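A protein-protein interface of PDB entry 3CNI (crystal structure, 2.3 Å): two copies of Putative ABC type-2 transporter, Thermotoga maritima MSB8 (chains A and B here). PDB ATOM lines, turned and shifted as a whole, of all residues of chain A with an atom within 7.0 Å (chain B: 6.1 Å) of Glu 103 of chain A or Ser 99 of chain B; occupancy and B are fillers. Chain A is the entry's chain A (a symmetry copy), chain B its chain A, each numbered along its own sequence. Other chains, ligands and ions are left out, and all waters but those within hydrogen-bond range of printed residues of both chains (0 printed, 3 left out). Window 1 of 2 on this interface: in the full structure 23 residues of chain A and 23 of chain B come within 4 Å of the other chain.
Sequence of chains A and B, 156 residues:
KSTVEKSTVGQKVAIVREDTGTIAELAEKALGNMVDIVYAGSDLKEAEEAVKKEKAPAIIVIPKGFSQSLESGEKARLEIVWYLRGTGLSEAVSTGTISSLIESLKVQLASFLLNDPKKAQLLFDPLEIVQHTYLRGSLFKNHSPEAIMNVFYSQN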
ATOM      1  N   MET A  34     -20.516   7.006 -40.217  1.00  0.00           N
ATOM      2  CA  MET A  34     -21.411   6.095 -39.523  1.00  0.00           C
ATOM      3  C   MET A  34     -22.884   6.295 -39.837  1.00  0.00           C
ATOM      4  O   MET A  34     -23.717   5.600 -39.290  1.00  0.00           O
ATOM      5  CB  MET A  34     -21.265   6.258 -38.027  1.00  0.00           C
ATOM      6  CG  MET A  34     -19.923   5.862 -37.416  1.00  0.00           C
ATOM      7  SD  MET A  34     -19.979   6.186 -35.440  1.00  0.00           S
ATOM      8  CE  MET A  34     -20.118   8.141 -35.177  1.00  0.00           C
ATOM      9  N   ILE A  98     -28.935   6.479 -33.178  1.00  0.00           N
ATOM     10  CA  ILE A  98     -28.158   7.751 -33.224  1.00  0.00           C
ATOM     11  C   ILE A  98     -27.497   8.011 -31.861  1.00  0.00           C
ATOM     12  O   ILE A  98     -26.354   8.481 -31.761  1.00  0.00           O
ATOM     13  CB  ILE A  98     -29.040   8.931 -33.776  1.00  0.00           C
ATOM     14  CG1 ILE A  98     -29.231   8.697 -35.280  1.00  0.00           C
ATOM     15  CG2 ILE A  98     -28.484  10.289 -33.523  1.00  0.00           C
ATOM     16  CD1 ILE A  98     -30.503   9.312 -35.854  1.00  0.00           C
ATOM     17  N   SER A  99     -28.178   7.626 -30.803  1.00  0.00           N
ATOM     18  CA  SER A  99     -27.600   7.798 -29.480  1.00  0.00           C
ATOM     19  C   SER A  99     -26.339   6.971 -29.335  1.00  0.00           C
ATOM     20  O   SER A  99     -25.367   7.362 -28.758  1.00  0.00           O
ATOM     21  CB  SER A  99     -28.547   7.320 -28.397  1.00  0.00           C
ATOM     22  OG  SER A  99     -29.642   8.139 -28.382  1.00  0.00           O
ATOM     23  N   SER A 100     -26.462   5.759 -29.784  1.00  0.00           N
ATOM     24  CA  SER A 100     -25.366   4.811 -29.876  1.00  0.00           C
ATOM     25  C   SER A 100     -24.209   5.385 -30.680  1.00  0.00           C
ATOM     26  O   SER A 100     -23.030   5.219 -30.360  1.00  0.00           O
ATOM     27  CB  SER A 100     -25.907   3.570 -30.539  1.00  0.00           C
ATOM     28  OG  SER A 100     -24.937   2.610 -30.588  1.00  0.00           O
ATOM     29  N   LEU A 101     -24.552   6.113 -31.728  1.00  0.00           N
ATOM     30  CA  LEU A 101     -23.515   6.731 -32.590  1.00  0.00           C
ATOM     31  C   LEU A 101     -22.801   7.886 -31.886  1.00  0.00           C
ATOM     32  O   LEU A 101     -21.623   8.074 -32.064  1.00  0.00           O
ATOM     33  CB  LEU A 101     -24.098   7.188 -33.952  1.00  0.00           C
ATOM     34  CG  LEU A 101     -24.746   6.074 -34.792  1.00  0.00           C
ATOM     35  CD1 LEU A 101     -25.335   6.643 -36.077  1.00  0.00           C
ATOM     36  CD2 LEU A 101     -23.774   4.948 -35.082  1.00  0.00           C
ATOM     37  N   ILE A 102     -23.512   8.655 -31.077  1.00  0.00           N
ATOM     38  CA  ILE A 102     -22.908   9.739 -30.329  1.00  0.00           C
ATOM     39  C   ILE A 102     -21.892   9.157 -29.300  1.00  0.00           C
ATOM     40  O   ILE A 102     -20.824   9.735 -29.024  1.00  0.00           O
ATOM     41  CB  ILE A 102     -23.994  10.603 -29.604  1.00  0.00           C
ATOM     42  CG1 ILE A 102     -24.886  11.332 -30.623  1.00  0.00           C
ATOM     43  CG2 ILE A 102     -23.353  11.574 -28.658  1.00  0.00           C
ATOM     44  CD1 ILE A 102     -24.170  11.647 -31.881  1.00  0.00           C
ATOM     45  N   GLU A 103     -22.239   8.014 -28.720  1.00  0.00           N
ATOM     46  CA  GLU A 103     -21.321   7.352 -27.735  1.00  0.00           C
ATOM     47  C   GLU A 103     -20.086   7.003 -28.475  1.00  0.00           C
ATOM     48  O   GLU A 103     -18.954   7.218 -28.035  1.00  0.00           O
ATOM     49  CB  GLU A 103     -21.935   6.098 -27.121  1.00  0.00           C
ATOM     50  CG  GLU A 103     -23.051   6.376 -26.178  1.00  0.00           C
ATOM     51  CD  GLU A 103     -22.606   7.158 -24.956  1.00  0.00           C
ATOM     52  OE1 GLU A 103     -21.380   7.256 -24.700  1.00  0.00           O
ATOM     53  OE2 GLU A 103     -23.479   7.686 -24.252  1.00  0.00           O
ATOM     54  N   SER A 104     -20.287   6.499 -29.659  1.00  0.00           N
ATOM     55  CA  SER A 104     -19.117   5.985 -30.415  1.00  0.00           C
ATOM     56  C   SER A 104     -18.174   7.121 -30.843  1.00  0.00           C
ATOM     57  O   SER A 104     -16.963   6.980 -30.940  1.00  0.00           O
ATOM     58  CB  SER A 104     -19.643   5.148 -31.603  1.00  0.00           C
ATOM     59  OG  SER A 104     -18.597   4.962 -32.500  1.00  0.00           O
ATOM     60  N   LEU A 105     -18.739   8.285 -31.052  1.00  0.00           N
ATOM     61  CA  LEU A 105     -17.982   9.470 -31.434  1.00  0.00           C
ATOM     62  C   LEU A 105     -17.038   9.910 -30.307  1.00  0.00           C
ATOM     63  O   LEU A 105     -15.931  10.417 -30.506  1.00  0.00           O
ATOM     64  CB  LEU A 105     -18.944  10.610 -31.787  1.00  0.00           C
ATOM     65  CG  LEU A 105     -18.284  11.981 -31.977  1.00  0.00           C
ATOM     66  CD1 LEU A 105     -17.199  12.014 -33.183  1.00  0.00           C
ATOM     67  CD2 LEU A 105     -19.355  13.066 -32.062  1.00  0.00           C
ATOM     68  N   LYS A 106     -17.489   9.662 -29.089  1.00  0.00           N
ATOM     69  CA  LYS A 106     -16.748  10.091 -27.942  1.00  0.00           C
ATOM     70  C   LYS A 106     -15.452   9.317 -27.909  1.00  0.00           C
ATOM     71  O   LYS A 106     -14.388   9.871 -27.582  1.00  0.00           O
ATOM     72  CB  LYS A 106     -17.508   9.770 -26.683  1.00  0.00           C
ATOM     73  CG  LYS A 106     -18.833  10.552 -26.503  1.00  0.00           C
ATOM     74  CD  LYS A 106     -19.454  10.112 -25.199  1.00  0.00           C
ATOM     75  CE  LYS A 106     -20.806  10.781 -25.001  1.00  0.00           C
ATOM     76  NZ  LYS A 106     -21.512  10.044 -23.932  1.00  0.00           N
ATOM     77  N   VAL A 107     -15.601   8.012 -28.168  1.00  0.00           N
ATOM     78  CA  VAL A 107     -14.482   7.098 -28.316  1.00  0.00           C
ATOM     79  C   VAL A 107     -13.524   7.538 -29.491  1.00  0.00           C
ATOM     80  O   VAL A 107     -12.291   7.516 -29.388  1.00  0.00           O
ATOM     81  CB  VAL A 107     -14.982   5.591 -28.518  1.00  0.00           C
ATOM     82  CG1 VAL A 107     -13.768   4.654 -28.828  1.00  0.00           C
ATOM     83  CG2 VAL A 107     -15.741   5.090 -27.307  1.00  0.00           C
ATOM     84  N   GLN A 108     -14.112   7.966 -30.596  1.00  0.00           N
ATOM     85  CA  GLN A 108     -13.335   8.348 -31.756  1.00  0.00           C
ATOM     86  C   GLN A 108     -12.708   9.730 -31.595  1.00  0.00           C
ATOM     87  O   GLN A 108     -12.011  10.198 -32.498  1.00  0.00           O
ATOM     88  CB  GLN A 108     -14.140   8.309 -33.051  1.00  0.00           C
ATOM     89  CG  GLN A 108     -14.674   6.942 -33.450  1.00  0.00           C
ATOM     90  CD  GLN A 108     -15.664   7.003 -34.626  1.00  0.00           C
ATOM     91  OE1 GLN A 108     -15.269   7.217 -35.762  1.00  0.00           O
ATOM     92  NE2 GLN A 108     -16.964   6.826 -34.343  1.00  0.00           N
ATOM     93  N   PHE A 124     -13.568  10.646 -20.540  1.00  0.00           N
ATOM     94  CA  PHE A 124     -14.760   9.904 -20.244  1.00  0.00           C
ATOM     95  C   PHE A 124     -16.024  10.644 -20.602  1.00  0.00           C
ATOM     96  O   PHE A 124     -17.002  10.043 -20.933  1.00  0.00           O
ATOM     97  CB  PHE A 124     -14.793   9.526 -18.786  1.00  0.00           C
ATOM     98  CG  PHE A 124     -13.732   8.586 -18.391  1.00  0.00           C
ATOM     99  CD1 PHE A 124     -12.474   9.027 -18.099  1.00  0.00           C
ATOM    100  CD2 PHE A 124     -13.985   7.259 -18.293  1.00  0.00           C
ATOM    101  CE1 PHE A 124     -11.490   8.147 -17.734  1.00  0.00           C
ATOM    102  CE2 PHE A 124     -13.003   6.387 -17.930  1.00  0.00           C
ATOM    103  CZ  PHE A 124     -11.756   6.836 -17.648  1.00  0.00           C
ATOM    104  N   LEU A 127     -18.430  15.428 -24.121  1.00  0.00           N
ATOM    105  CA  LEU A 127     -19.468  16.146 -24.849  1.00  0.00           C
ATOM    106  C   LEU A 127     -20.601  16.571 -23.921  1.00  0.00           C
ATOM    107  O   LEU A 127     -21.006  15.820 -23.035  1.00  0.00           O
ATOM    108  CB  LEU A 127     -20.018  15.285 -25.988  1.00  0.00           C
ATOM    109  CG  LEU A 127     -19.010  14.847 -27.054  1.00  0.00           C
ATOM    110  CD1 LEU A 127     -19.671  13.937 -28.077  1.00  0.00           C
ATOM    111  CD2 LEU A 127     -18.386  16.058 -27.732  1.00  0.00           C
ATOM    112  N   TRP B  82     -18.659  -1.216 -12.892  1.00  0.00           N
ATOM    113  CA  TRP B  82     -17.448  -0.950 -13.642  1.00  0.00           C
ATOM    114  C   TRP B  82     -16.237  -1.169 -12.813  1.00  0.00           C
ATOM    115  O   TRP B  82     -16.240  -0.863 -11.657  1.00  0.00           O
ATOM    116  CB  TRP B  82     -17.412   0.500 -14.139  1.00  0.00           C
ATOM    117  CG  TRP B  82     -18.534   0.924 -15.044  1.00  0.00           C
ATOM    118  CD1 TRP B  82     -19.714   1.538 -14.672  1.00  0.00           C
ATOM    119  CD2 TRP B  82     -18.539   0.873 -16.469  1.00  0.00           C
ATOM    120  NE1 TRP B  82     -20.438   1.835 -15.777  1.00  0.00           N
ATOM    121  CE2 TRP B  82     -19.745   1.441 -16.897  1.00  0.00           C
ATOM    122  CE3 TRP B  82     -17.626   0.426 -17.426  1.00  0.00           C
ATOM    123  CZ2 TRP B  82     -20.078   1.557 -18.256  1.00  0.00           C
ATOM    124  CZ3 TRP B  82     -17.975   0.523 -18.762  1.00  0.00           C
ATOM    125  CH2 TRP B  82     -19.171   1.109 -19.160  1.00  0.00           C
ATOM    126  N   SER B  94     -13.525   1.628 -23.245  1.00  0.00           N
ATOM    127  CA  SER B  94     -14.526   0.672 -22.682  1.00  0.00           C
ATOM    128  C   SER B  94     -15.797   1.325 -22.249  1.00  0.00           C
ATOM    129  O   SER B  94     -16.903   0.810 -22.472  1.00  0.00           O
ATOM    130  CB  SER B  94     -13.997  -0.083 -21.454  1.00  0.00           C
ATOM    131  OG  SER B  94     -12.938  -0.966 -21.794  1.00  0.00           O
ATOM    132  N   THR B  95     -15.656   2.429 -21.543  1.00  0.00           N
ATOM    133  CA  THR B  95     -16.829   3.168 -21.084  1.00  0.00           C
ATOM    134  C   THR B  95     -17.749   3.589 -22.205  1.00  0.00           C
ATOM    135  O   THR B  95     -18.927   3.297 -22.193  1.00  0.00           O
ATOM    136  CB  THR B  95     -16.425   4.409 -20.304  1.00  0.00           C
ATOM    137  OG1 THR B  95     -15.717   3.987 -19.138  1.00  0.00           O
ATOM    138  CG2 THR B  95     -17.625   5.101 -19.780  1.00  0.00           C
ATOM    139  N   GLY B  96     -17.193   4.291 -23.177  1.00  0.00           N
ATOM    140  CA  GLY B  96     -17.926   4.714 -24.363  1.00  0.00           C
ATOM    141  C   GLY B  96     -18.473   3.562 -25.176  1.00  0.00           C
ATOM    142  O   GLY B  96     -19.589   3.603 -25.662  1.00  0.00           O
ATOM    143  N   THR B  97     -17.676   2.530 -25.352  1.00  0.00           N
ATOM    144  CA  THR B  97     -18.106   1.352 -26.155  1.00  0.00           C
ATOM    145  C   THR B  97     -19.240   0.597 -25.533  1.00  0.00           C
ATOM    146  O   THR B  97     -20.157   0.249 -26.209  1.00  0.00           O
ATOM    147  CB  THR B  97     -16.941   0.355 -26.438  1.00  0.00           C
ATOM    148  OG1 THR B  97     -15.891   1.069 -27.044  1.00  0.00           O
ATOM    149  CG2 THR B  97     -17.329  -0.666 -27.412  1.00  0.00           C
ATOM    150  N   ILE B  98     -19.173   0.343 -24.243  1.00  0.00           N
ATOM    151  CA  ILE B  98     -20.240  -0.404 -23.518  1.00  0.00           C
ATOM    152  C   ILE B  98     -21.519   0.447 -23.445  1.00  0.00           C
ATOM    153  O   ILE B  98     -22.648  -0.047 -23.575  1.00  0.00           O
ATOM    154  CB  ILE B  98     -19.715  -0.942 -22.137  1.00  0.00           C
ATOM    155  CG1 ILE B  98     -18.751  -2.099 -22.432  1.00  0.00           C
ATOM    156  CG2 ILE B  98     -20.784  -1.377 -21.195  1.00  0.00           C
ATOM    157  CD1 ILE B  98     -17.695  -2.326 -21.355  1.00  0.00           C
ATOM    158  N   SER B  99     -21.344   1.746 -23.322  1.00  0.00           N
ATOM    159  CA  SER B  99     -22.503   2.622 -23.289  1.00  0.00           C
ATOM    160  C   SER B  99     -23.266   2.550 -24.597  1.00  0.00           C
ATOM    161  O   SER B  99     -24.460   2.560 -24.655  1.00  0.00           O
ATOM    162  CB  SER B  99     -22.096   4.072 -23.115  1.00  0.00           C
ATOM    163  OG  SER B  99     -21.540   4.224 -21.875  1.00  0.00           O
ATOM    164  N   SER B 100     -22.501   2.604 -25.644  1.00  0.00           N
ATOM    165  CA  SER B 100     -22.972   2.428 -27.005  1.00  0.00           C
ATOM    166  C   SER B 100     -23.717   1.110 -27.163  1.00  0.00           C
ATOM    167  O   SER B 100     -24.745   1.003 -27.836  1.00  0.00           O
ATOM    168  CB  SER B 100     -21.762   2.462 -27.903  1.00  0.00           C
ATOM    169  OG  SER B 100     -22.150   2.374 -29.210  1.00  0.00           O
ATOM    170  N   LEU B 101     -23.211   0.089 -26.494  1.00  0.00           N
ATOM    171  CA  LEU B 101     -23.849  -1.247 -26.563  1.00  0.00           C
ATOM    172  C   LEU B 101     -25.185  -1.283 -25.818  1.00  0.00           C
ATOM    173  O   LEU B 101     -26.103  -1.937 -26.244  1.00  0.00           O
ATOM    174  CB  LEU B 101     -22.901  -2.364 -26.051  1.00  0.00           C
ATOM    175  CG  LEU B 101     -21.567  -2.484 -26.808  1.00  0.00           C
ATOM    176  CD1 LEU B 101     -20.693  -3.567 -26.188  1.00  0.00           C
ATOM    177  CD2 LEU B 101     -21.779  -2.728 -28.289  1.00  0.00           C
ATOM    178  N   ILE B 102     -25.297  -0.569 -24.709  1.00  0.00           N
ATOM    179  CA  ILE B 102     -26.540  -0.501 -23.968  1.00  0.00           C
ATOM    180  C   ILE B 102     -27.625   0.205 -24.837  1.00  0.00           C
ATOM    181  O   ILE B 102     -28.820  -0.143 -24.816  1.00  0.00           O
ATOM    182  CB  ILE B 102     -26.350   0.249 -22.607  1.00  0.00           C
ATOM    183  CG1 ILE B 102     -25.422  -0.543 -21.669  1.00  0.00           C
ATOM    184  CG2 ILE B 102     -27.675   0.512 -21.957  1.00  0.00           C
ATOM    185  CD1 ILE B 102     -25.503  -2.005 -21.894  1.00  0.00           C
ATOM    186  N   GLU B 103     -27.203   1.214 -25.591  1.00  0.00           N
ATOM    187  CA  GLU B 103     -28.159   1.944 -26.487  1.00  0.00           C
ATOM    188  C   GLU B 103     -28.652   0.957 -27.475  1.00  0.00           C
ATOM    189  O   GLU B 103     -29.842   0.846 -27.780  1.00  0.00           O
ATOM    190  CB  GLU B 103     -27.500   3.119 -27.205  1.00  0.00           C
ATOM    191  CG  GLU B 103     -27.173   4.261 -26.311  1.00  0.00           C
ATOM    192  CD  GLU B 103     -28.406   4.898 -25.698  1.00  0.00           C
ATOM    193  OE1 GLU B 103     -29.539   4.632 -26.172  1.00  0.00           O
ATOM    194  OE2 GLU B 103     -28.249   5.660 -24.733  1.00  0.00           O
ATOM    195  N   SER B 104     -27.735   0.169 -27.960  1.00  0.00           N
ATOM    196  CA  SER B 104     -28.108  -0.754 -29.062  1.00  0.00           C
ATOM    197  C   SER B 104     -29.073  -1.850 -28.583  1.00  0.00           C
ATOM    198  O   SER B 104     -29.934  -2.338 -29.300  1.00  0.00           O
ATOM    199  CB  SER B 104     -26.806  -1.313 -29.681  1.00  0.00           C
ATOM    200  OG  SER B 104     -27.134  -2.420 -30.456  1.00  0.00           O
ATOM    201  N   GLN B 131     -25.534   2.586 -12.365  1.00  0.00           N
ATOM    202  CA  GLN B 131     -24.103   2.326 -12.563  1.00  0.00           C
ATOM    203  C   GLN B 131     -23.358   2.437 -11.281  1.00  0.00           C
ATOM    204  O   GLN B 131     -23.669   3.244 -10.429  1.00  0.00           O
ATOM    205  CB  GLN B 131     -23.522   3.273 -13.599  1.00  0.00           C
ATOM    206  CG  GLN B 131     -24.315   3.396 -14.858  1.00  0.00           C
ATOM    207  CD  GLN B 131     -23.569   4.144 -15.948  1.00  0.00           C
ATOM    208  OE1 GLN B 131     -22.445   3.841 -16.263  1.00  0.00           O
ATOM    209  NE2 GLN B 131     -24.207   5.126 -16.526  1.00  0.00           N
ATOM    210  N   GLU B 146     -17.935   8.427 -15.487  1.00  0.00           N
ATOM    211  CA  GLU B 146     -17.939   9.856 -15.844  1.00  0.00           C
ATOM    212  C   GLU B 146     -18.033  10.690 -14.580  1.00  0.00           C
ATOM    213  O   GLU B 146     -17.304  11.681 -14.378  1.00  0.00           O
ATOM    214  CB  GLU B 146     -19.130  10.207 -16.688  1.00  0.00           C
ATOM    215  CG  GLU B 146     -19.181   9.594 -18.125  1.00  0.00           C
ATOM    216  CD  GLU B 146     -19.859   8.186 -18.297  1.00  0.00           C
ATOM    217  OE1 GLU B 146     -19.889   7.267 -17.410  1.00  0.00           O
ATOM    218  OE2 GLU B 146     -20.302   7.993 -19.423  1.00  0.00           O
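Ser 99 of chain A touches Glu 103 of chain B, and with the chains exchanged Glu 103 of chain A touches Ser 99 of chain B.
Ser 100 of chain B touches its own counterpart, Ser 100 of chain A.
Ser 100 of chain A touches Glu 103 of chain B, and with the chains exchanged Glu 103 of chain A touches Ser 100 of chain B.
Of the 10 pairs that touch across the chains among the printed residues, 5 have their exchanged pair printed and touching as well.
Among the printed residues, pairs that only touch across the chains: Phe 124 of chain A with Glu 146 of chain B, Ser 99 of chain A with Glu 103 of chain B, Glu 103 of chain A with Ser 99 of chain B, Val 107 of chain A with Gly 96 of chain B, Ser 100 of chain A with Glu 103 of chain B, Glu 103 of chain A with Gly 96 of chain B, Glu 103 of chain A with Ser 100 of chain B, Val 107 of chain A with Thr 97 of chain B and Phe 124 of chain A with Thr 95 of chain B.
Of the 14 printed residues of chain A, 5 touch a printed residue of chain B.
Hydrophobic or aromatic side chains of chain A within 4 Å of the printed part of chain B: Val 107 and Phe 124.
Along chain A the printed residues that touch a printed residue of chain B span positions 99 to 124.
Printed residues of chain B within 4 Å of Ser 99 of chain A: Glu 103 (3.6 Å).
Glu 103 of chain A touches three residues of chain B.
Lys 106 of chain A touches none of the printed residues of chain B.
Ser 99 of chain B touches one residue of chain A.
Printed residues of chain A within 4 Å of Ser 100 of chain B: Ser 100 (3.1 Å) and Glu 103 (3.7 Å).
The nearest residue of chain A that does not touch Ser 99 of chain B is Ser 100 of chain A (5.8 Å).
The side-chain hydroxyl (OG) of Ser 99 of chain B sits close to the backbone carbonyl oxygen (O) of Thr 95 of chain B (2.8 Å).
The side-chain carboxylate (OE1) of Glu 103 of chain A is in salt-bridge range of the side-chain amino group (NZ) of Lys 106 of chain A (2.9 Å).
The side-chain hydroxyl (OG) of Ser 100 of chain B is in hydrogen-bond range of the side-chain hydroxyl (OG) of Ser 100 of chain A (3.1 Å).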
